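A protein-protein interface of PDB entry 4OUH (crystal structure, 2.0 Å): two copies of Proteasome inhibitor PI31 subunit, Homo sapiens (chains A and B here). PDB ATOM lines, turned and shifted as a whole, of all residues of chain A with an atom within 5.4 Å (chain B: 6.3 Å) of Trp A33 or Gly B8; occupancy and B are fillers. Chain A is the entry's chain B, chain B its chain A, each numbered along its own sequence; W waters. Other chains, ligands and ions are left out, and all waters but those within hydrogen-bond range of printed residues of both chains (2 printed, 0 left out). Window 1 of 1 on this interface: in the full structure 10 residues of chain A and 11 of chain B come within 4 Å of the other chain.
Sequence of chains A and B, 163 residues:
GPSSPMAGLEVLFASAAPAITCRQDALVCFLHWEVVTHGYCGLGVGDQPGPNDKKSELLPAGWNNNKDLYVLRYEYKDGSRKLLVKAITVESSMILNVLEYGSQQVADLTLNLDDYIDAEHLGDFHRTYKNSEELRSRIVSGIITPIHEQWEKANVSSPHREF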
ATOM      1  N   MET A   6      19.465 -16.827  -8.385  1.00  0.00           N
ATOM      2  CA  MET A   6      18.365 -17.736  -8.117  1.00  0.00           C
ATOM      3  C   MET A   6      17.922 -17.590  -6.662  1.00  0.00           C
ATOM      4  O   MET A   6      17.344 -18.508  -6.079  1.00  0.00           O
ATOM      5  CB  MET A   6      18.748 -19.177  -8.439  1.00  0.00           C
ATOM      6  CG  MET A   6      18.714 -19.496  -9.927  1.00  0.00           C
ATOM      7  SD  MET A   6      17.038 -19.701 -10.556  1.00  0.00           S
ATOM      8  CE  MET A   6      16.690 -21.369 -10.003  1.00  0.00           C
ATOM      9  N   ALA A   7      18.201 -16.422  -6.091  1.00  0.00           N
ATOM     10  CA  ALA A   7      17.748 -16.095  -4.746  1.00  0.00           C
ATOM     11  C   ALA A   7      16.235 -16.211  -4.698  1.00  0.00           C
ATOM     12  O   ALA A   7      15.529 -15.646  -5.537  1.00  0.00           O
ATOM     13  CB  ALA A   7      18.190 -14.693  -4.367  1.00  0.00           C
ATOM     14  N   GLY A   8      15.740 -16.970  -3.728  1.00  0.00           N
ATOM     15  CA  GLY A   8      14.316 -17.228  -3.620  1.00  0.00           C
ATOM     16  C   GLY A   8      13.970 -18.686  -3.856  1.00  0.00           C
ATOM     17  O   GLY A   8      12.889 -19.139  -3.480  1.00  0.00           O
ATOM     18  N   LEU A   9      14.882 -19.426  -4.479  1.00  0.00           N
ATOM     19  CA  LEU A   9      14.628 -20.832  -4.784  1.00  0.00           C
ATOM     20  C   LEU A   9      14.398 -21.630  -3.505  1.00  0.00           C
ATOM     21  O   LEU A   9      13.498 -22.464  -3.444  1.00  0.00           O
ATOM     22  CB  LEU A   9      15.773 -21.442  -5.597  1.00  0.00           C
ATOM     23  CG  LEU A   9      15.608 -22.931  -5.924  1.00  0.00           C
ATOM     24  CD1 LEU A   9      14.404 -23.175  -6.836  1.00  0.00           C
ATOM     25  CD2 LEU A   9      16.881 -23.518  -6.530  1.00  0.00           C
ATOM     26  N   VAL A  11      13.205 -20.523  -0.705  1.00  0.00           N
ATOM     27  CA  VAL A  11      11.900 -20.138  -0.182  1.00  0.00           C
ATOM     28  C   VAL A  11      10.790 -20.788  -1.003  1.00  0.00           C
ATOM     29  O   VAL A  11       9.813 -21.299  -0.454  1.00  0.00           O
ATOM     30  CB  VAL A  11      11.709 -18.606  -0.177  1.00  0.00           C
ATOM     31  CG1 VAL A  11      10.423 -18.239   0.547  1.00  0.00           C
ATOM     32  CG2 VAL A  11      12.896 -17.920   0.481  1.00  0.00           C
ATOM     33  N   LEU A  12      10.947 -20.770  -2.323  1.00  0.00           N
ATOM     34  CA  LEU A  12       9.983 -21.410  -3.217  1.00  0.00           C
ATOM     35  C   LEU A  12       9.885 -22.912  -2.944  1.00  0.00           C
ATOM     36  O   LEU A  12       8.786 -23.474  -2.876  1.00  0.00           O
ATOM     37  CB  LEU A  12      10.359 -21.171  -4.684  1.00  0.00           C
ATOM     38  CG  LEU A  12       9.391 -21.747  -5.725  1.00  0.00           C
ATOM     39  CD1 LEU A  12       8.088 -20.963  -5.739  1.00  0.00           C
ATOM     40  CD2 LEU A  12      10.012 -21.779  -7.117  1.00  0.00           C
ATOM     41  N   VAL A  28      10.836 -29.045 -12.170  1.00  0.00           N
ATOM     42  CA  VAL A  28       9.903 -28.012 -12.614  1.00  0.00           C
ATOM     43  C   VAL A  28       9.907 -26.818 -11.652  1.00  0.00           C
ATOM     44  O   VAL A  28       9.750 -25.670 -12.069  1.00  0.00           O
ATOM     45  CB  VAL A  28       8.479 -28.583 -12.796  1.00  0.00           C
ATOM     46  CG1 VAL A  28       7.454 -27.469 -12.977  1.00  0.00           C
ATOM     47  CG2 VAL A  28       8.445 -29.536 -13.987  1.00  0.00           C
ATOM     48  N   CYS A  29      10.103 -27.096 -10.368  1.00  0.00           N
ATOM     49  CA  CYS A  29      10.226 -26.041  -9.368  1.00  0.00           C
ATOM     50  C   CYS A  29      11.426 -25.148  -9.692  1.00  0.00           C
ATOM     51  O   CYS A  29      11.324 -23.920  -9.676  1.00  0.00           O
ATOM     52  CB  CYS A  29      10.373 -26.654  -7.973  1.00  0.00           C
ATOM     53  SG  CYS A  29      10.554 -25.451  -6.638  1.00  0.00           S
ATOM     54  N   PHE A  30      12.555 -25.780 -10.002  1.00  0.00           N
ATOM     55  CA  PHE A  30      13.782 -25.076 -10.375  1.00  0.00           C
ATOM     56  C   PHE A  30      13.571 -24.269 -11.657  1.00  0.00           C
ATOM     57  O   PHE A  30      13.960 -23.100 -11.741  1.00  0.00           O
ATOM     58  CB  PHE A  30      14.915 -26.093 -10.577  1.00  0.00           C
ATOM     59  CG  PHE A  30      16.292 -25.483 -10.639  1.00  0.00           C
ATOM     60  CD1 PHE A  30      16.749 -24.868 -11.798  1.00  0.00           C
ATOM     61  CD2 PHE A  30      17.141 -25.556  -9.546  1.00  0.00           C
ATOM     62  CE1 PHE A  30      18.019 -24.317 -11.854  1.00  0.00           C
ATOM     63  CE2 PHE A  30      18.411 -25.008  -9.594  1.00  0.00           C
ATOM     64  CZ  PHE A  30      18.851 -24.390 -10.749  1.00  0.00           C
ATOM     65  N   LEU A  31      12.958 -24.905 -12.654  1.00  0.00           N
ATOM     66  CA  LEU A  31      12.679 -24.265 -13.937  1.00  0.00           C
ATOM     67  C   LEU A  31      11.777 -23.043 -13.772  1.00  0.00           C
ATOM     68  O   LEU A  31      12.015 -21.994 -14.378  1.00  0.00           O
ATOM     69  CB  LEU A  31      12.032 -25.267 -14.901  1.00  0.00           C
ATOM     70  CG  LEU A  31      11.412 -24.705 -16.184  1.00  0.00           C
ATOM     71  CD1 LEU A  31      12.466 -24.044 -17.058  1.00  0.00           C
ATOM     72  CD2 LEU A  31      10.682 -25.799 -16.958  1.00  0.00           C
ATOM     73  N   HIS A  32      10.740 -23.192 -12.956  1.00  0.00           N
ATOM     74  CA  HIS A  32       9.812 -22.106 -12.673  1.00  0.00           C
ATOM     75  C   HIS A  32      10.557 -20.890 -12.139  1.00  0.00           C
ATOM     76  O   HIS A  32      10.314 -19.759 -12.571  1.00  0.00           O
ATOM     77  CB  HIS A  32       8.770 -22.558 -11.651  1.00  0.00           C
ATOM     78  CG  HIS A  32       7.877 -21.457 -11.163  1.00  0.00           C
ATOM     79  ND1 HIS A  32       6.835 -20.957 -11.911  1.00  0.00           N
ATOM     80  CD2 HIS A  32       7.870 -20.768  -9.996  1.00  0.00           C
ATOM     81  CE1 HIS A  32       6.223 -20.002 -11.227  1.00  0.00           C
ATOM     82  NE2 HIS A  32       6.833 -19.870 -10.063  1.00  0.00           N
ATOM     83  N   TRP A  33      11.468 -21.119 -11.202  1.00  0.00           N
ATOM     84  CA  TRP A  33      12.181 -20.002 -10.599  1.00  0.00           C
ATOM     85  C   TRP A  33      13.167 -19.358 -11.565  1.00  0.00           C
ATOM     86  O   TRP A  33      13.433 -18.159 -11.480  1.00  0.00           O
ATOM     87  CB  TRP A  33      12.870 -20.391  -9.286  1.00  0.00           C
ATOM     88  CG  TRP A  33      13.078 -19.185  -8.408  1.00  0.00           C
ATOM     89  CD1 TRP A  33      14.261 -18.696  -7.934  1.00  0.00           C
ATOM     90  CD2 TRP A  33      12.061 -18.295  -7.940  1.00  0.00           C
ATOM     91  NE1 TRP A  33      14.039 -17.563  -7.182  1.00  0.00           N
ATOM     92  CE2 TRP A  33      12.695 -17.298  -7.171  1.00  0.00           C
ATOM     93  CE3 TRP A  33      10.670 -18.252  -8.086  1.00  0.00           C
ATOM     94  CZ2 TRP A  33      11.984 -16.268  -6.554  1.00  0.00           C
ATOM     95  CZ3 TRP A  33       9.969 -17.228  -7.475  1.00  0.00           C
ATOM     96  CH2 TRP A  33      10.626 -16.252  -6.716  1.00  0.00           C
ATOM     97  N   GLU A  34      13.707 -20.153 -12.485  1.00  0.00           N
ATOM     98  CA  GLU A  34      14.540 -19.600 -13.550  1.00  0.00           C
ATOM     99  C   GLU A  34      13.736 -18.632 -14.407  1.00  0.00           C
ATOM    100  O   GLU A  34      14.238 -17.581 -14.817  1.00  0.00           O
ATOM    101  CB  GLU A  34      15.124 -20.710 -14.433  1.00  0.00           C
ATOM    102  CG  GLU A  34      16.430 -21.311 -13.919  1.00  0.00           C
ATOM    103  CD  GLU A  34      17.621 -20.361 -14.035  1.00  0.00           C
ATOM    104  OE1 GLU A  34      17.430 -19.179 -14.393  1.00  0.00           O
ATOM    105  OE2 GLU A  34      18.758 -20.801 -13.771  1.00  0.00           O
ATOM    106  N   VAL A  35      12.485 -18.994 -14.671  1.00  0.00           N
ATOM    107  CA  VAL A  35      11.608 -18.174 -15.497  1.00  0.00           C
ATOM    108  C   VAL A  35      11.197 -16.907 -14.758  1.00  0.00           C
ATOM    109  O   VAL A  35      11.228 -15.809 -15.321  1.00  0.00           O
ATOM    110  CB  VAL A  35      10.357 -18.959 -15.948  1.00  0.00           C
ATOM    111  CG1 VAL A  35       9.388 -18.047 -16.684  1.00  0.00           C
ATOM    112  CG2 VAL A  35      10.765 -20.118 -16.840  1.00  0.00           C
ATOM    113  N   VAL A  36      10.821 -17.058 -13.491  1.00  0.00           N
ATOM    114  CA  VAL A  36      10.443 -15.903 -12.678  1.00  0.00           C
ATOM    115  C   VAL A  36      11.604 -14.921 -12.495  1.00  0.00           C
ATOM    116  O   VAL A  36      11.427 -13.711 -12.652  1.00  0.00           O
ATOM    117  CB  VAL A  36       9.882 -16.320 -11.306  1.00  0.00           C
ATOM    118  CG1 VAL A  36       9.698 -15.097 -10.412  1.00  0.00           C
ATOM    119  CG2 VAL A  36       8.562 -17.048 -11.477  1.00  0.00           C
ATOM    120  N   THR A  37      12.790 -15.436 -12.179  1.00  0.00           N
ATOM    121  CA  THR A  37      13.934 -14.556 -11.934  1.00  0.00           C
ATOM    122  C   THR A  37      14.416 -13.864 -13.204  1.00  0.00           C
ATOM    123  O   THR A  37      15.193 -12.908 -13.143  1.00  0.00           O
ATOM    124  CB  THR A  37      15.115 -15.293 -11.271  1.00  0.00           C
ATOM    125  OG1 THR A  37      15.504 -16.413 -12.075  1.00  0.00           O
ATOM    126  CG2 THR A  37      14.732 -15.765  -9.877  1.00  0.00           C
ATOM    127  N   HIS A  38      13.952 -14.344 -14.354  1.00  0.00           N
ATOM    128  CA  HIS A  38      14.274 -13.690 -15.616  1.00  0.00           C
ATOM    129  C   HIS A  38      13.138 -12.813 -16.131  1.00  0.00           C
ATOM    130  O   HIS A  38      13.052 -12.527 -17.324  1.00  0.00           O
ATOM    131  CB  HIS A  38      14.737 -14.706 -16.663  1.00  0.00           C
ATOM    132  CG  HIS A  38      16.141 -15.178 -16.445  1.00  0.00           C
ATOM    133  ND1 HIS A  38      16.454 -16.209 -15.585  1.00  0.00           N
ATOM    134  CD2 HIS A  38      17.317 -14.736 -16.947  1.00  0.00           C
ATOM    135  CE1 HIS A  38      17.762 -16.393 -15.582  1.00  0.00           C
ATOM    136  NE2 HIS A  38      18.309 -15.513 -16.400  1.00  0.00           N
ATOM    137  N   GLU A  57       4.390 -14.903  -8.461  1.00  0.00           N
ATOM    138  CA  GLU A  57       5.691 -15.567  -8.409  1.00  0.00           C
ATOM    139  C   GLU A  57       5.551 -17.016  -7.979  1.00  0.00           C
ATOM    140  O   GLU A  57       6.394 -17.852  -8.298  1.00  0.00           O
ATOM    141  CB  GLU A  57       6.614 -14.878  -7.402  1.00  0.00           C
ATOM    142  CG  GLU A  57       7.095 -13.496  -7.791  1.00  0.00           C
ATOM    143  CD  GLU A  57       8.039 -12.916  -6.755  1.00  0.00           C
ATOM    144  OE1 GLU A  57       8.133 -13.491  -5.649  1.00  0.00           O
ATOM    145  OE2 GLU A  57       8.687 -11.890  -7.044  1.00  0.00           O
ATOM    146  N   MET B   6      13.689  -7.762  -6.444  1.00  0.00           N
ATOM    147  CA  MET B   6      13.045  -8.216  -5.236  1.00  0.00           C
ATOM    148  C   MET B   6      12.193  -9.439  -5.550  1.00  0.00           C
ATOM    149  O   MET B   6      11.271  -9.775  -4.805  1.00  0.00           O
ATOM    150  CB  MET B   6      12.220  -7.091  -4.623  1.00  0.00           C
ATOM    151  CG  MET B   6      13.060  -6.057  -3.873  1.00  0.00           C
ATOM    152  SD  MET B   6      13.826  -6.680  -2.360  1.00  0.00           S
ATOM    153  CE  MET B   6      12.434  -6.599  -1.232  1.00  0.00           C
ATOM    154  N   ALA B   7      12.527 -10.100  -6.659  1.00  0.00           N
ATOM    155  CA  ALA B   7      11.908 -11.364  -7.023  1.00  0.00           C
ATOM    156  C   ALA B   7      12.088 -12.331  -5.871  1.00  0.00           C
ATOM    157  O   ALA B   7      13.213 -12.592  -5.428  1.00  0.00           O
ATOM    158  CB  ALA B   7      12.535 -11.917  -8.287  1.00  0.00           C
ATOM    159  N   GLY B   8      10.969 -12.842  -5.377  1.00  0.00           N
ATOM    160  CA  GLY B   8      10.980 -13.720  -4.227  1.00  0.00           C
ATOM    161  C   GLY B   8      10.250 -13.110  -3.047  1.00  0.00           C
ATOM    162  O   GLY B   8       9.865 -13.825  -2.125  1.00  0.00           O
ATOM    163  N   LEU B   9      10.061 -11.791  -3.067  1.00  0.00           N
ATOM    164  CA  LEU B   9       9.365 -11.116  -1.969  1.00  0.00           C
ATOM    165  C   LEU B   9       7.957 -11.673  -1.796  1.00  0.00           C
ATOM    166  O   LEU B   9       7.511 -11.922  -0.674  1.00  0.00           O
ATOM    167  CB  LEU B   9       9.307  -9.599  -2.187  1.00  0.00           C
ATOM    168  CG  LEU B   9       8.485  -8.816  -1.149  1.00  0.00           C
ATOM    169  CD1 LEU B   9       9.013  -9.036   0.266  1.00  0.00           C
ATOM    170  CD2 LEU B   9       8.441  -7.330  -1.479  1.00  0.00           C
ATOM    171  N   GLU B  10       7.262 -11.886  -2.908  1.00  0.00           N
ATOM    172  CA  GLU B  10       5.905 -12.421  -2.847  1.00  0.00           C
ATOM    173  C   GLU B  10       5.886 -13.814  -2.227  1.00  0.00           C
ATOM    174  O   GLU B  10       4.986 -14.154  -1.458  1.00  0.00           O
ATOM    175  CB  GLU B  10       5.269 -12.464  -4.237  1.00  0.00           C
ATOM    176  CG  GLU B  10       3.795 -12.829  -4.205  1.00  0.00           C
ATOM    177  CD  GLU B  10       3.204 -13.039  -5.584  1.00  0.00           C
ATOM    178  OE1 GLU B  10       3.905 -12.775  -6.584  1.00  0.00           O
ATOM    179  OE2 GLU B  10       2.036 -13.477  -5.661  1.00  0.00           O
ATOM    180  N   VAL B  11       6.884 -14.620  -2.575  1.00  0.00           N
ATOM    181  CA  VAL B  11       6.988 -15.977  -2.055  1.00  0.00           C
ATOM    182  C   VAL B  11       7.349 -15.938  -0.574  1.00  0.00           C
ATOM    183  O   VAL B  11       6.780 -16.677   0.234  1.00  0.00           O
ATOM    184  CB  VAL B  11       8.046 -16.793  -2.820  1.00  0.00           C
ATOM    185  CG1 VAL B  11       8.091 -18.221  -2.300  1.00  0.00           C
ATOM    186  CG2 VAL B  11       7.748 -16.780  -4.310  1.00  0.00           C
ATOM    187  N   LEU B  12       8.294 -15.069  -0.226  1.00  0.00           N
ATOM    188  CA  LEU B  12       8.683 -14.873   1.169  1.00  0.00           C
ATOM    189  C   LEU B  12       7.481 -14.454   2.008  1.00  0.00           C
ATOM    190  O   LEU B  12       7.219 -15.032   3.064  1.00  0.00           O
ATOM    191  CB  LEU B  12       9.787 -13.816   1.285  1.00  0.00           C
ATOM    192  CG  LEU B  12      10.251 -13.504   2.713  1.00  0.00           C
ATOM    193  CD1 LEU B  12      11.014 -14.682   3.301  1.00  0.00           C
ATOM    194  CD2 LEU B  12      11.091 -12.232   2.764  1.00  0.00           C
ATOM    195  N   PHE B  13       6.755 -13.448   1.525  1.00  0.00           N
ATOM    196  CA  PHE B  13       5.597 -12.909   2.235  1.00  0.00           C
ATOM    197  C   PHE B  13       4.552 -13.993   2.481  1.00  0.00           C
ATOM    198  O   PHE B  13       3.977 -14.083   3.569  1.00  0.00           O
ATOM    199  CB  PHE B  13       4.983 -11.745   1.449  1.00  0.00           C
ATOM    200  CG  PHE B  13       3.951 -10.961   2.219  1.00  0.00           C
ATOM    201  CD1 PHE B  13       2.616 -11.344   2.213  1.00  0.00           C
ATOM    202  CD2 PHE B  13       4.315  -9.826   2.933  1.00  0.00           C
ATOM    203  CE1 PHE B  13       1.665 -10.620   2.918  1.00  0.00           C
ATOM    204  CE2 PHE B  13       3.371  -9.096   3.637  1.00  0.00           C
ATOM    205  CZ  PHE B  13       2.044  -9.493   3.629  1.00  0.00           C
ATOM    206  N   TRP B  33      14.293  -9.335   2.787  1.00  0.00           N
ATOM    207  CA  TRP B  33      14.504  -9.757   1.407  1.00  0.00           C
ATOM    208  C   TRP B  33      15.455  -8.830   0.654  1.00  0.00           C
ATOM    209  O   TRP B  33      16.183  -9.268  -0.240  1.00  0.00           O
ATOM    210  CB  TRP B  33      13.183  -9.919   0.649  1.00  0.00           C
ATOM    211  CG  TRP B  33      13.339 -10.838  -0.519  1.00  0.00           C
ATOM    212  CD1 TRP B  33      13.152 -10.539  -1.837  1.00  0.00           C
ATOM    213  CD2 TRP B  33      13.759 -12.207  -0.470  1.00  0.00           C
ATOM    214  NE1 TRP B  33      13.415 -11.647  -2.612  1.00  0.00           N
ATOM    215  CE2 TRP B  33      13.788 -12.679  -1.797  1.00  0.00           C
ATOM    216  CE3 TRP B  33      14.104 -13.078   0.568  1.00  0.00           C
ATOM    217  CZ2 TRP B  33      14.152 -13.991  -2.108  1.00  0.00           C
ATOM    218  CZ3 TRP B  33      14.466 -14.373   0.257  1.00  0.00           C
ATOM    219  CH2 TRP B  33      14.486 -14.818  -1.069  1.00  0.00           C
HETATM  220  O   HOH W   1       8.117 -10.130  -5.359  1.00  0.00           O
HETATM  221  O   HOH W   2      15.750 -13.127  -6.654  1.00  0.00           O
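The side-chain carboxylate (OE1) of Glu A57 is in hydrogen-bond range of the backbone NH (N) of Gly B8, 2.9 Å away.
N of Glu A57 is in hydrogen-bond range of OE1 of Glu B10 (2.9 Å).
O of Ala B7 lies within hydrogen-bond range of NE1 of Trp B33, at 3.0 Å.
The backbone carbonyl oxygen (O) of Ala A7 is in hydrogen-bond range of the indole nitrogen (NE1) of Trp A33.
The backbone carbonyl oxygen (O) of Glu A57 lies within hydrogen-bond range of a ring nitrogen (NE2) of His A32 (2.7 Å).
OG1 of Thr A37 is in hydrogen-bond range of O of Trp A33, at 2.8 Å.
Ala A7 touches Ala B7 (O to O, 3.8 Å).
CZ2 of Trp B33 touches C of Ala A7, at 3.997 Å.
Gly A8 touches Trp B33.
Val B11 touches Val A11 (CG1 to CG1, 3.7 Å).
CH2 of Trp B33 touches CG2 of Val A11, 3.8 Å away.
Leu A12 touches Val B11.
Trp A33 touches Gly B8.
CG2 of Val B11 touches CH2 of Trp A33, at 3.8 Å.
Leu B9 touches Glu A57.
Glu A57 touches Val B11.
Of the printed residues of chain B, Gly A8 touches Trp B33.
His A32 touches none of the printed residues of chain B.
Of the printed residues of chain B, Trp A33 touches Ala B7, Gly B8 and Val B11.
Glu A34 touches none of the printed residues of chain B.
Of the printed residues of chain A, Glu B10 touches Glu A57 (2.9 Å).
Of the printed residues of chain A, Val B11 touches Val A11, Leu A12, Trp A33 and Glu A57.
The nearest printed residue of chain B that does not touch Trp A33 is Trp B33 (5.4 Å).
The nearest residue of chain A that does not touch Gly B8 is Gly A8 (4.9 Å).
The nearest printed residue of chain B that does not touch Leu A12 is Leu B12 (6.6 Å).
Of the 18 printed residues of chain A, 6 touch a printed residue of chain B.
Hydrophobic or aromatic side chains of chain A within 4 Å of the printed part of chain B: Val A11 and Trp A33.
Hydrophobic or aromatic side chains of chain B within 4 Å of the printed part of chain A: Val B11 and Trp B33.
Among the printed residues, no Asp or Glu carboxylate lies within 4 Å of a Lys or Arg side-chain nitrogen of the other chain.
Ala A7 touches its own counterpart, Ala B7.
Ala A7 touches Trp B33, and with the chains exchanged Trp A33 touches Ala B7.
Gly A8 touches Trp B33, and with the chains exchanged Trp A33 touches Gly B8.
Val B11 touches its own counterpart, Val A11.
7 positions are printed for both chains.
Of the 15 pairs that touch across the chains among the printed residues, 10 have their exchanged pair printed and touching as well.
Water W1 lies within hydrogen-bond range of OE2 of Glu A57, N of Glu B10, O of Met B6 and N of Leu B9.
Water W2 lies within hydrogen-bond range of O of Ala A7 (2.8 Å) and O of Ala B7 (2.9 Å).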
